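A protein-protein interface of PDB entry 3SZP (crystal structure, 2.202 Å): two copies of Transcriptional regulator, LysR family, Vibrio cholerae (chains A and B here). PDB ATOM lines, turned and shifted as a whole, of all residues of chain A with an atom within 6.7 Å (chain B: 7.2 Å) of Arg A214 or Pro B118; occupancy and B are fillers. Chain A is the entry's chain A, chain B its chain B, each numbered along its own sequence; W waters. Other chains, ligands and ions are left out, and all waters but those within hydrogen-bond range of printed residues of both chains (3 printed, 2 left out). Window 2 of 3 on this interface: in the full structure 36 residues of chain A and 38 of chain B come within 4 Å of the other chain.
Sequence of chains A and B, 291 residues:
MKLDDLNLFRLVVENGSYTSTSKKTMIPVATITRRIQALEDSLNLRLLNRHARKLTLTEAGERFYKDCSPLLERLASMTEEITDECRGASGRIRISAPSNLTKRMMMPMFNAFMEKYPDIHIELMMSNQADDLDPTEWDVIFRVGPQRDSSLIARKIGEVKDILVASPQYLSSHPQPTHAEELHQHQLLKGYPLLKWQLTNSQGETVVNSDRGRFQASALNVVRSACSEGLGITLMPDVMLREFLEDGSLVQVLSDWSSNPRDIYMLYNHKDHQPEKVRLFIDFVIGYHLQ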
ATOM      1  N   TYR A 170     -13.875 -16.434  13.184  1.00  0.00           N
ATOM      2  CA  TYR A 170     -14.061 -15.065  12.688  1.00  0.00           C
ATOM      3  C   TYR A 170     -13.163 -14.084  13.456  1.00  0.00           C
ATOM      4  O   TYR A 170     -12.509 -13.218  12.864  1.00  0.00           O
ATOM      5  CB  TYR A 170     -15.523 -14.617  12.778  1.00  0.00           C
ATOM      6  CG  TYR A 170     -15.716 -13.162  12.398  1.00  0.00           C
ATOM      7  CD1 TYR A 170     -15.830 -12.778  11.061  1.00  0.00           C
ATOM      8  CD2 TYR A 170     -15.762 -12.173  13.367  1.00  0.00           C
ATOM      9  CE1 TYR A 170     -15.988 -11.449  10.704  1.00  0.00           C
ATOM     10  CE2 TYR A 170     -15.916 -10.842  13.023  1.00  0.00           C
ATOM     11  CZ  TYR A 170     -16.035 -10.490  11.690  1.00  0.00           C
ATOM     12  OH  TYR A 170     -16.188  -9.176  11.346  1.00  0.00           O
ATOM     13  N   HIS A 174     -10.479 -11.146  12.447  1.00  0.00           N
ATOM     14  CA  HIS A 174     -11.048  -9.809  12.578  1.00  0.00           C
ATOM     15  C   HIS A 174     -11.115  -9.491  14.052  1.00  0.00           C
ATOM     16  O   HIS A 174     -12.097  -9.833  14.710  1.00  0.00           O
ATOM     17  CB  HIS A 174     -12.472  -9.768  12.025  1.00  0.00           C
ATOM     18  CG  HIS A 174     -12.589 -10.289  10.632  1.00  0.00           C
ATOM     19  ND1 HIS A 174     -12.645 -11.636  10.348  1.00  0.00           N
ATOM     20  CD2 HIS A 174     -12.637  -9.645   9.442  1.00  0.00           C
ATOM     21  CE1 HIS A 174     -12.727 -11.800   9.040  1.00  0.00           C
ATOM     22  NE2 HIS A 174     -12.723 -10.609   8.468  1.00  0.00           N
ATOM     23  N   HIS A 186     -17.009  -4.272  10.845  1.00  0.00           N
ATOM     24  CA  HIS A 186     -17.109  -5.727  10.876  1.00  0.00           C
ATOM     25  C   HIS A 186     -18.174  -6.279   9.952  1.00  0.00           C
ATOM     26  O   HIS A 186     -19.035  -5.533   9.488  1.00  0.00           O
ATOM     27  CB  HIS A 186     -17.388  -6.195  12.299  1.00  0.00           C
ATOM     28  CG  HIS A 186     -16.163  -6.263  13.137  1.00  0.00           C
ATOM     29  ND1 HIS A 186     -15.398  -7.403  13.232  1.00  0.00           N
ATOM     30  CD2 HIS A 186     -15.548  -5.324  13.896  1.00  0.00           C
ATOM     31  CE1 HIS A 186     -14.365  -7.168  14.021  1.00  0.00           C
ATOM     32  NE2 HIS A 186     -14.437  -5.915  14.439  1.00  0.00           N
ATOM     33  N   GLN A 187     -18.108  -7.591   9.709  1.00  0.00           N
ATOM     34  CA  GLN A 187     -19.141  -8.301   8.952  1.00  0.00           C
ATOM     35  C   GLN A 187     -20.317  -8.604   9.868  1.00  0.00           C
ATOM     36  O   GLN A 187     -20.183  -9.360  10.826  1.00  0.00           O
ATOM     37  CB  GLN A 187     -18.595  -9.600   8.361  1.00  0.00           C
ATOM     38  CG  GLN A 187     -17.525  -9.370   7.320  1.00  0.00           C
ATOM     39  CD  GLN A 187     -17.858  -8.170   6.439  1.00  0.00           C
ATOM     40  OE1 GLN A 187     -18.785  -8.218   5.630  1.00  0.00           O
ATOM     41  NE2 GLN A 187     -17.107  -7.066   6.615  1.00  0.00           N
ATOM     42  N   LEU A 188     -21.467  -8.006   9.587  1.00  0.00           N
ATOM     43  CA  LEU A 188     -22.630  -8.232  10.445  1.00  0.00           C
ATOM     44  C   LEU A 188     -23.641  -9.205   9.839  1.00  0.00           C
ATOM     45  O   LEU A 188     -23.824  -9.246   8.622  1.00  0.00           O
ATOM     46  CB  LEU A 188     -23.284  -6.906  10.832  1.00  0.00           C
ATOM     47  CG  LEU A 188     -22.287  -5.901  11.402  1.00  0.00           C
ATOM     48  CD1 LEU A 188     -23.011  -4.651  11.876  1.00  0.00           C
ATOM     49  CD2 LEU A 188     -21.469  -6.528  12.565  1.00  0.00           C
ATOM     50  N   LEU A 189     -24.285  -9.987  10.702  1.00  0.00           N
ATOM     51  CA  LEU A 189     -25.255 -10.993  10.299  1.00  0.00           C
ATOM     52  C   LEU A 189     -26.524 -10.714  11.085  1.00  0.00           C
ATOM     53  O   LEU A 189     -26.517 -10.747  12.318  1.00  0.00           O
ATOM     54  CB  LEU A 189     -24.759 -12.399  10.629  1.00  0.00           C
ATOM     55  CG  LEU A 189     -23.302 -12.689  10.249  1.00  0.00           C
ATOM     56  CD1 LEU A 189     -22.808 -13.989  10.920  1.00  0.00           C
ATOM     57  CD2 LEU A 189     -23.144 -12.785   8.728  1.00  0.00           C
ATOM     58  N   LYS A 190     -27.608 -10.428  10.373  1.00  0.00           N
ATOM     59  CA  LYS A 190     -28.809  -9.939  11.034  1.00  0.00           C
ATOM     60  C   LYS A 190     -30.057 -10.710  10.617  1.00  0.00           C
ATOM     61  O   LYS A 190     -30.281 -10.965   9.424  1.00  0.00           O
ATOM     62  CB  LYS A 190     -28.996  -8.438  10.787  1.00  0.00           C
ATOM     63  CG  LYS A 190     -27.761  -7.549  11.128  1.00  0.00           C
ATOM     64  CD  LYS A 190     -28.177  -6.085  11.140  1.00  0.00           C
ATOM     65  CE  LYS A 190     -27.074  -5.108  11.513  1.00  0.00           C
ATOM     66  NZ  LYS A 190     -27.643  -3.717  11.557  1.00  0.00           N
ATOM     67  N   ARG A 212     -26.847  -2.891   6.740  1.00  0.00           N
ATOM     68  CA  ARG A 212     -27.634  -3.958   6.128  1.00  0.00           C
ATOM     69  C   ARG A 212     -27.120  -5.348   6.473  1.00  0.00           C
ATOM     70  O   ARG A 212     -27.902  -6.297   6.596  1.00  0.00           O
ATOM     71  CB  ARG A 212     -27.648  -3.790   4.612  1.00  0.00           C
ATOM     72  CG  ARG A 212     -28.527  -2.655   4.161  1.00  0.00           C
ATOM     73  CD  ARG A 212     -29.945  -2.903   4.626  1.00  0.00           C
ATOM     74  NE  ARG A 212     -30.767  -3.471   3.561  1.00  0.00           N
ATOM     75  CZ  ARG A 212     -32.003  -3.922   3.740  1.00  0.00           C
ATOM     76  NH1 ARG A 212     -32.549  -3.883   4.953  1.00  0.00           N
ATOM     77  NH2 ARG A 212     -32.691  -4.418   2.714  1.00  0.00           N
ATOM     78  N   GLY A 213     -25.802  -5.469   6.609  1.00  0.00           N
ATOM     79  CA  GLY A 213     -25.217  -6.750   6.947  1.00  0.00           C
ATOM     80  C   GLY A 213     -24.757  -7.553   5.748  1.00  0.00           C
ATOM     81  O   GLY A 213     -25.329  -7.481   4.645  1.00  0.00           O
ATOM     82  N   ARG A 214     -23.690  -8.308   5.966  1.00  0.00           N
ATOM     83  CA  ARG A 214     -23.224  -9.293   5.008  1.00  0.00           C
ATOM     84  C   ARG A 214     -24.338 -10.293   4.704  1.00  0.00           C
ATOM     85  O   ARG A 214     -24.466 -10.768   3.582  1.00  0.00           O
ATOM     86  CB  ARG A 214     -22.036 -10.036   5.601  1.00  0.00           C
ATOM     87  CG  ARG A 214     -21.406 -11.036   4.658  1.00  0.00           C
ATOM     88  CD  ARG A 214     -20.362 -11.837   5.399  1.00  0.00           C
ATOM     89  NE  ARG A 214     -19.499 -12.562   4.482  1.00  0.00           N
ATOM     90  CZ  ARG A 214     -18.327 -13.080   4.823  1.00  0.00           C
ATOM     91  NH1 ARG A 214     -17.900 -12.946   6.072  1.00  0.00           N
ATOM     92  NH2 ARG A 214     -17.590 -13.716   3.917  1.00  0.00           N
ATOM     93  N   PHE A 215     -25.140 -10.604   5.718  1.00  0.00           N
ATOM     94  CA  PHE A 215     -26.223 -11.579   5.604  1.00  0.00           C
ATOM     95  C   PHE A 215     -27.402 -10.982   6.365  1.00  0.00           C
ATOM     96  O   PHE A 215     -27.270 -10.627   7.544  1.00  0.00           O
ATOM     97  CB  PHE A 215     -25.783 -12.930   6.222  1.00  0.00           C
ATOM     98  CG  PHE A 215     -26.810 -14.050   6.117  1.00  0.00           C
ATOM     99  CD1 PHE A 215     -27.460 -14.325   4.915  1.00  0.00           C
ATOM    100  CD2 PHE A 215     -27.091 -14.869   7.231  1.00  0.00           C
ATOM    101  CE1 PHE A 215     -28.394 -15.361   4.808  1.00  0.00           C
ATOM    102  CE2 PHE A 215     -28.022 -15.923   7.136  1.00  0.00           C
ATOM    103  CZ  PHE A 215     -28.678 -16.170   5.921  1.00  0.00           C
ATOM    104  N   GLN A 216     -28.533 -10.824   5.682  1.00  0.00           N
ATOM    105  CA  GLN A 216     -29.791 -10.472   6.346  1.00  0.00           C
ATOM    106  C   GLN A 216     -30.831 -11.521   5.998  1.00  0.00           C
ATOM    107  O   GLN A 216     -30.977 -11.898   4.835  1.00  0.00           O
ATOM    108  CB  GLN A 216     -30.294  -9.075   5.947  1.00  0.00           C
ATOM    109  CG  GLN A 216     -31.589  -8.676   6.676  1.00  0.00           C
ATOM    110  CD  GLN A 216     -32.359  -7.531   5.991  1.00  0.00           C
ATOM    111  OE1 GLN A 216     -31.838  -6.428   5.833  1.00  0.00           O
ATOM    112  NE2 GLN A 216     -33.592  -7.799   5.582  1.00  0.00           N
ATOM    113  N   GLY A 230     -18.416 -18.677  10.889  1.00  0.00           N
ATOM    114  CA  GLY A 230     -17.385 -17.658  10.969  1.00  0.00           C
ATOM    115  C   GLY A 230     -17.578 -16.505  10.005  1.00  0.00           C
ATOM    116  O   GLY A 230     -16.624 -15.885   9.559  1.00  0.00           O
ATOM    117  N   LEU A 231     -18.823 -16.195   9.683  1.00  0.00           N
ATOM    118  CA  LEU A 231     -19.071 -15.182   8.672  1.00  0.00           C
ATOM    119  C   LEU A 231     -19.288 -13.794   9.255  1.00  0.00           C
ATOM    120  O   LEU A 231     -19.443 -12.838   8.504  1.00  0.00           O
ATOM    121  CB  LEU A 231     -20.241 -15.581   7.777  1.00  0.00           C
ATOM    122  CG  LEU A 231     -20.031 -16.822   6.913  1.00  0.00           C
ATOM    123  CD1 LEU A 231     -21.385 -17.265   6.315  1.00  0.00           C
ATOM    124  CD2 LEU A 231     -18.950 -16.630   5.832  1.00  0.00           C
ATOM    125  N   GLY A 232     -19.276 -13.682  10.582  1.00  0.00           N
ATOM    126  CA  GLY A 232     -19.385 -12.380  11.213  1.00  0.00           C
ATOM    127  C   GLY A 232     -20.095 -12.355  12.554  1.00  0.00           C
ATOM    128  O   GLY A 232     -20.284 -13.393  13.188  1.00  0.00           O
ATOM    129  N   ARG B  92     -25.350  -6.506  -2.958  1.00  0.00           N
ATOM    130  CA  ARG B  92     -26.467  -7.242  -2.402  1.00  0.00           C
ATOM    131  C   ARG B  92     -27.235  -8.066  -3.417  1.00  0.00           C
ATOM    132  O   ARG B  92     -27.573  -7.599  -4.500  1.00  0.00           O
ATOM    133  CB  ARG B  92     -27.403  -6.249  -1.706  1.00  0.00           C
ATOM    134  CG  ARG B  92     -28.586  -6.852  -0.966  1.00  0.00           C
ATOM    135  CD  ARG B  92     -28.833  -6.080   0.339  1.00  0.00           C
ATOM    136  NE  ARG B  92     -28.134  -6.726   1.445  1.00  0.00           N
ATOM    137  CZ  ARG B  92     -28.647  -6.904   2.660  1.00  0.00           C
ATOM    138  NH1 ARG B  92     -29.877  -6.457   2.958  1.00  0.00           N
ATOM    139  NH2 ARG B  92     -27.922  -7.536   3.569  1.00  0.00           N
ATOM    140  N   ASN B 111     -23.817 -20.594   3.092  1.00  0.00           N
ATOM    141  CA  ASN B 111     -22.668 -20.293   3.946  1.00  0.00           C
ATOM    142  C   ASN B 111     -21.349 -20.409   3.171  1.00  0.00           C
ATOM    143  O   ASN B 111     -20.491 -19.527   3.248  1.00  0.00           O
ATOM    144  CB  ASN B 111     -22.654 -21.190   5.202  1.00  0.00           C
ATOM    145  CG  ASN B 111     -23.672 -20.736   6.264  1.00  0.00           C
ATOM    146  OD1 ASN B 111     -24.029 -19.561   6.324  1.00  0.00           O
ATOM    147  ND2 ASN B 111     -24.146 -21.666   7.082  1.00  0.00           N
ATOM    148  N   PHE B 113     -21.004 -20.185   0.035  1.00  0.00           N
ATOM    149  CA  PHE B 113     -20.961 -19.152  -0.988  1.00  0.00           C
ATOM    150  C   PHE B 113     -20.421 -17.868  -0.391  1.00  0.00           C
ATOM    151  O   PHE B 113     -19.532 -17.227  -0.960  1.00  0.00           O
ATOM    152  CB  PHE B 113     -22.348 -18.880  -1.574  1.00  0.00           C
ATOM    153  CG  PHE B 113     -22.375 -17.714  -2.537  1.00  0.00           C
ATOM    154  CD1 PHE B 113     -21.893 -17.856  -3.835  1.00  0.00           C
ATOM    155  CD2 PHE B 113     -22.875 -16.481  -2.145  1.00  0.00           C
ATOM    156  CE1 PHE B 113     -21.915 -16.786  -4.731  1.00  0.00           C
ATOM    157  CE2 PHE B 113     -22.904 -15.402  -3.039  1.00  0.00           C
ATOM    158  CZ  PHE B 113     -22.418 -15.559  -4.326  1.00  0.00           C
ATOM    159  N   MET B 114     -20.981 -17.499   0.759  1.00  0.00           N
ATOM    160  CA  MET B 114     -20.642 -16.240   1.406  1.00  0.00           C
ATOM    161  C   MET B 114     -19.175 -16.202   1.859  1.00  0.00           C
ATOM    162  O   MET B 114     -18.502 -15.172   1.723  1.00  0.00           O
ATOM    163  CB  MET B 114     -21.605 -15.957   2.575  1.00  0.00           C
ATOM    164  CG  MET B 114     -23.004 -15.511   2.104  1.00  0.00           C
ATOM    165  SD  MET B 114     -24.090 -14.906   3.417  1.00  0.00           S
ATOM    166  CE  MET B 114     -24.729 -16.431   4.062  1.00  0.00           C
ATOM    167  N   GLU B 115     -18.693 -17.322   2.388  1.00  0.00           N
ATOM    168  CA  GLU B 115     -17.282 -17.443   2.756  1.00  0.00           C
ATOM    169  C   GLU B 115     -16.410 -17.241   1.519  1.00  0.00           C
ATOM    170  O   GLU B 115     -15.345 -16.627   1.593  1.00  0.00           O
ATOM    171  CB  GLU B 115     -16.989 -18.820   3.379  1.00  0.00           C
ATOM    172  CG  GLU B 115     -15.486 -19.089   3.693  1.00  0.00           C
ATOM    173  N   LYS B 116     -16.861 -17.755   0.379  1.00  0.00           N
ATOM    174  CA  LYS B 116     -16.055 -17.652  -0.827  1.00  0.00           C
ATOM    175  C   LYS B 116     -16.016 -16.233  -1.363  1.00  0.00           C
ATOM    176  O   LYS B 116     -15.004 -15.797  -1.888  1.00  0.00           O
ATOM    177  CB  LYS B 116     -16.532 -18.610  -1.921  1.00  0.00           C
ATOM    178  CG  LYS B 116     -15.515 -18.771  -3.055  1.00  0.00           C
ATOM    179  CD  LYS B 116     -16.066 -19.605  -4.190  1.00  0.00           C
ATOM    180  CE  LYS B 116     -15.007 -19.816  -5.250  1.00  0.00           C
ATOM    181  NZ  LYS B 116     -13.641 -20.074  -4.649  1.00  0.00           N
ATOM    182  N   TYR B 117     -17.123 -15.516  -1.235  1.00  0.00           N
ATOM    183  CA  TYR B 117     -17.223 -14.179  -1.810  1.00  0.00           C
ATOM    184  C   TYR B 117     -17.643 -13.124  -0.788  1.00  0.00           C
ATOM    185  O   TYR B 117     -18.814 -12.776  -0.686  1.00  0.00           O
ATOM    186  CB  TYR B 117     -18.227 -14.190  -2.947  1.00  0.00           C
ATOM    187  CG  TYR B 117     -17.903 -15.143  -4.072  1.00  0.00           C
ATOM    188  CD1 TYR B 117     -16.908 -14.844  -4.990  1.00  0.00           C
ATOM    189  CD2 TYR B 117     -18.621 -16.325  -4.244  1.00  0.00           C
ATOM    190  CE1 TYR B 117     -16.621 -15.690  -6.048  1.00  0.00           C
ATOM    191  CE2 TYR B 117     -18.332 -17.190  -5.311  1.00  0.00           C
ATOM    192  CZ  TYR B 117     -17.339 -16.856  -6.203  1.00  0.00           C
ATOM    193  OH  TYR B 117     -17.042 -17.692  -7.256  1.00  0.00           O
ATOM    194  N   PRO B 118     -16.674 -12.598  -0.036  1.00  0.00           N
ATOM    195  CA  PRO B 118     -16.979 -11.636   1.029  1.00  0.00           C
ATOM    196  C   PRO B 118     -17.645 -10.327   0.568  1.00  0.00           C
ATOM    197  O   PRO B 118     -18.270  -9.665   1.393  1.00  0.00           O
ATOM    198  CB  PRO B 118     -15.605 -11.369   1.691  1.00  0.00           C
ATOM    199  CG  PRO B 118     -14.590 -11.873   0.726  1.00  0.00           C
ATOM    200  CD  PRO B 118     -15.241 -12.940  -0.109  1.00  0.00           C
ATOM    201  N   ASP B 119     -17.531  -9.958  -0.704  1.00  0.00           N
ATOM    202  CA  ASP B 119     -18.125  -8.702  -1.145  1.00  0.00           C
ATOM    203  C   ASP B 119     -19.552  -8.885  -1.682  1.00  0.00           C
ATOM    204  O   ASP B 119     -20.173  -7.928  -2.123  1.00  0.00           O
ATOM    205  CB  ASP B 119     -17.229  -7.987  -2.175  1.00  0.00           C
ATOM    206  CG  ASP B 119     -15.920  -7.484  -1.568  1.00  0.00           C
ATOM    207  OD1 ASP B 119     -15.927  -6.999  -0.413  1.00  0.00           O
ATOM    208  OD2 ASP B 119     -14.864  -7.578  -2.239  1.00  0.00           O
ATOM    209  N   ILE B 120     -20.063 -10.115  -1.650  1.00  0.00           N
ATOM    210  CA  ILE B 120     -21.447 -10.360  -2.038  1.00  0.00           C
ATOM    211  C   ILE B 120     -22.330 -10.558  -0.809  1.00  0.00           C
ATOM    212  O   ILE B 120     -22.086 -11.452  -0.012  1.00  0.00           O
ATOM    213  CB  ILE B 120     -21.583 -11.565  -2.980  1.00  0.00           C
ATOM    214  CG1 ILE B 120     -20.760 -11.349  -4.273  1.00  0.00           C
ATOM    215  CG2 ILE B 120     -23.062 -11.809  -3.307  1.00  0.00           C
ATOM    216  CD1 ILE B 120     -20.771 -12.563  -5.208  1.00  0.00           C
ATOM    217  N   HIS B 121     -23.358  -9.724  -0.675  1.00  0.00           N
ATOM    218  CA  HIS B 121     -24.251  -9.758   0.476  1.00  0.00           C
ATOM    219  C   HIS B 121     -25.597 -10.377   0.112  1.00  0.00           C
ATOM    220  O   HIS B 121     -26.172 -10.092  -0.948  1.00  0.00           O
ATOM    221  CB  HIS B 121     -24.436  -8.348   1.048  1.00  0.00           C
ATOM    222  CG  HIS B 121     -23.157  -7.708   1.484  1.00  0.00           C
ATOM    223  ND1 HIS B 121     -21.953  -8.384   1.492  1.00  0.00           N
ATOM    224  CD2 HIS B 121     -22.889  -6.459   1.935  1.00  0.00           C
ATOM    225  CE1 HIS B 121     -20.999  -7.578   1.921  1.00  0.00           C
ATOM    226  NE2 HIS B 121     -21.543  -6.407   2.211  1.00  0.00           N
ATOM    227  N   ILE B 122     -26.090 -11.243   0.991  1.00  0.00           N
ATOM    228  CA  ILE B 122     -27.320 -11.954   0.710  1.00  0.00           C
ATOM    229  C   ILE B 122     -28.429 -11.406   1.589  1.00  0.00           C
ATOM    230  O   ILE B 122     -28.243 -11.249   2.810  1.00  0.00           O
ATOM    231  CB  ILE B 122     -27.192 -13.457   0.994  1.00  0.00           C
ATOM    232  CG1 ILE B 122     -26.355 -14.144  -0.088  1.00  0.00           C
ATOM    233  CG2 ILE B 122     -28.592 -14.088   1.151  1.00  0.00           C
ATOM    234  CD1 ILE B 122     -26.091 -15.608   0.179  1.00  0.00           C
ATOM    235  N   GLU B 123     -29.554 -11.074   0.966  1.00  0.00           N
ATOM    236  CA  GLU B 123     -30.766 -10.767   1.706  1.00  0.00           C
ATOM    237  C   GLU B 123     -31.709 -11.940   1.441  1.00  0.00           C
ATOM    238  O   GLU B 123     -32.050 -12.219   0.294  1.00  0.00           O
ATOM    239  CB  GLU B 123     -31.366  -9.432   1.271  1.00  0.00           C
ATOM    240  CG  GLU B 123     -32.715  -9.125   1.932  1.00  0.00           C
ATOM    241  CD  GLU B 123     -33.346  -7.827   1.435  1.00  0.00           C
ATOM    242  OE1 GLU B 123     -32.611  -6.885   1.073  1.00  0.00           O
ATOM    243  OE2 GLU B 123     -34.582  -7.754   1.376  1.00  0.00           O
HETATM  244  O   HOH W   1     -14.771 -14.871   4.050  1.00  0.00           O
HETATM  245  O   HOH W   2     -20.335  -5.885   5.219  1.00  0.00           O
HETATM  246  O   HOH W   3     -17.722  -9.962   4.242  1.00  0.00           O
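The backbone carbonyl oxygen (O) of Leu A188 sits at hydrogen-bond distance from the backbone NH (N) of Arg A214. The backbone carbonyl oxygen (O) of Leu A188 sits at hydrogen-bond distance from the backbone NH (N) of Phe A215, 3.5 Å away. The backbone carbonyl oxygen (O) of Phe A215 sits at hydrogen-bond distance from the backbone NH (N) of Lys A190, 2.9 Å away. The side-chain amide oxygen (OE1) of Gln A216 lies within hydrogen-bond range of the guanidinium group (NH1) of Arg A212, at 2.8 Å. NH1 of Arg A214 is in hydrogen-bond range of O of Leu A231 (2.9 Å). The side-chain carboxylate of Glu B123 lies within salt-bridge range of the guanidinium group of Arg B92.
Hydrophobic or aromatic side chains of chain A within 4 Å of the printed part of chain B: Phe A215 and Leu A231. Printed residues of chain B that touch a printed residue of chain A: Arg B92, Asn B111, Met B114, Glu B115, Pro B118, His B121, Ile B122 and Glu B123. Hydrophobic or aromatic side chains of chain B within 4 Å of the printed part of chain A: Met B114, Pro B118, His B121 and Ile B122. Among the printed residues, 17 pairs touch across the chains.
No position is printed for both chains. Of the 17 pairs that touch across the chains among the printed residues, none has its exchanged pair printed and touching as well.
Water W3 lies within hydrogen-bond range of the side-chain amide oxygen (OE1) of Gln A187 (2.5 Å), the backbone carbonyl oxygen (O) of Pro B118 (2.9 Å) and the guanidinium group (NE) of Arg A214 (3.2 Å). Water W2 bridges OE1 of Gln A187 (2.8 Å) and NE2 of His B121 (3.3 Å). Water W1 bridges the guanidinium group (NH2) of Arg A214 (3.0 Å) and the backbone carbonyl oxygen (O) of Glu B115 (3.1 Å).
Tyr A170 touches none of the printed residues of chain B. Printed residues of chain B within 4 Å of Gly A213: Arg B92 (2.8 Å) and His B121 (3.8 Å). Arg A214 touches five residues of chain B. Of the printed residues of chain B, Phe A215 touches Met B114 and Ile B122. Printed residues of chain B within 4 Å of Gln A216: Arg B92, Ile B122 and Glu B123. Of chain A, only Arg A214 comes within 4 Å of Pro B118. Of the printed residues of chain A, Ile B122 touches Arg A214 (3.1 Å), Phe A215 (3.5 Å) and Gln A216 (2.9 Å). Of the printed residues of chain A, Glu B123 touches Arg A212 and Gln A216. The nearest residue of chain B that does not touch Arg A214 is Ile B120 (4.4 Å). The nearest residue of chain A that does not touch Pro B118 is Gln A187 (4.5 Å). The nearest printed residue of chain A that does not touch His B121 is Gln A187 (4.4 Å).
NH2 of Arg B92 lies within hydrogen-bond range of O of Arg A212, at 3.3 Å. NH2 of Arg A212 lies within salt-bridge range of OE1 of Glu B123. O of Gly A213 lies within hydrogen-bond range of NH2 of Arg B92. The guanidinium group of Arg A214 lies within hydrogen-bond range of the backbone carbonyl oxygen of Met B114, at 2.8 Å. The backbone carbonyl oxygen (O) of Arg A214 sits at hydrogen-bond distance from the backbone NH (N) of Ile B122, 3.1 Å away. The side-chain amide oxygen of Gln A216 is in hydrogen-bond range of the guanidinium group of Arg B92 (3.5 Å). The backbone NH (N) of Gln A216 is in hydrogen-bond range of the backbone carbonyl oxygen (O) of Ile B122, 2.9 Å away.
His B121 touches Gly A213. CA of Glu B115 touches NH2 of Arg A214, 3.9 Å away. Arg A214 touches Pro B118. His B121 touches Arg A214 (CA to O, 3.3 Å). Met B114 touches Phe A215 (CE to CD1, 3.6 Å). Phe A215 touches Ile B122. Gln A216 touches Glu B123 (O to CA, 3.3 Å). Leu A231 touches Asn B111. Met B114 touches Leu A231. CD2 of Leu A231 touches N of Glu B115 (3.5 Å).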
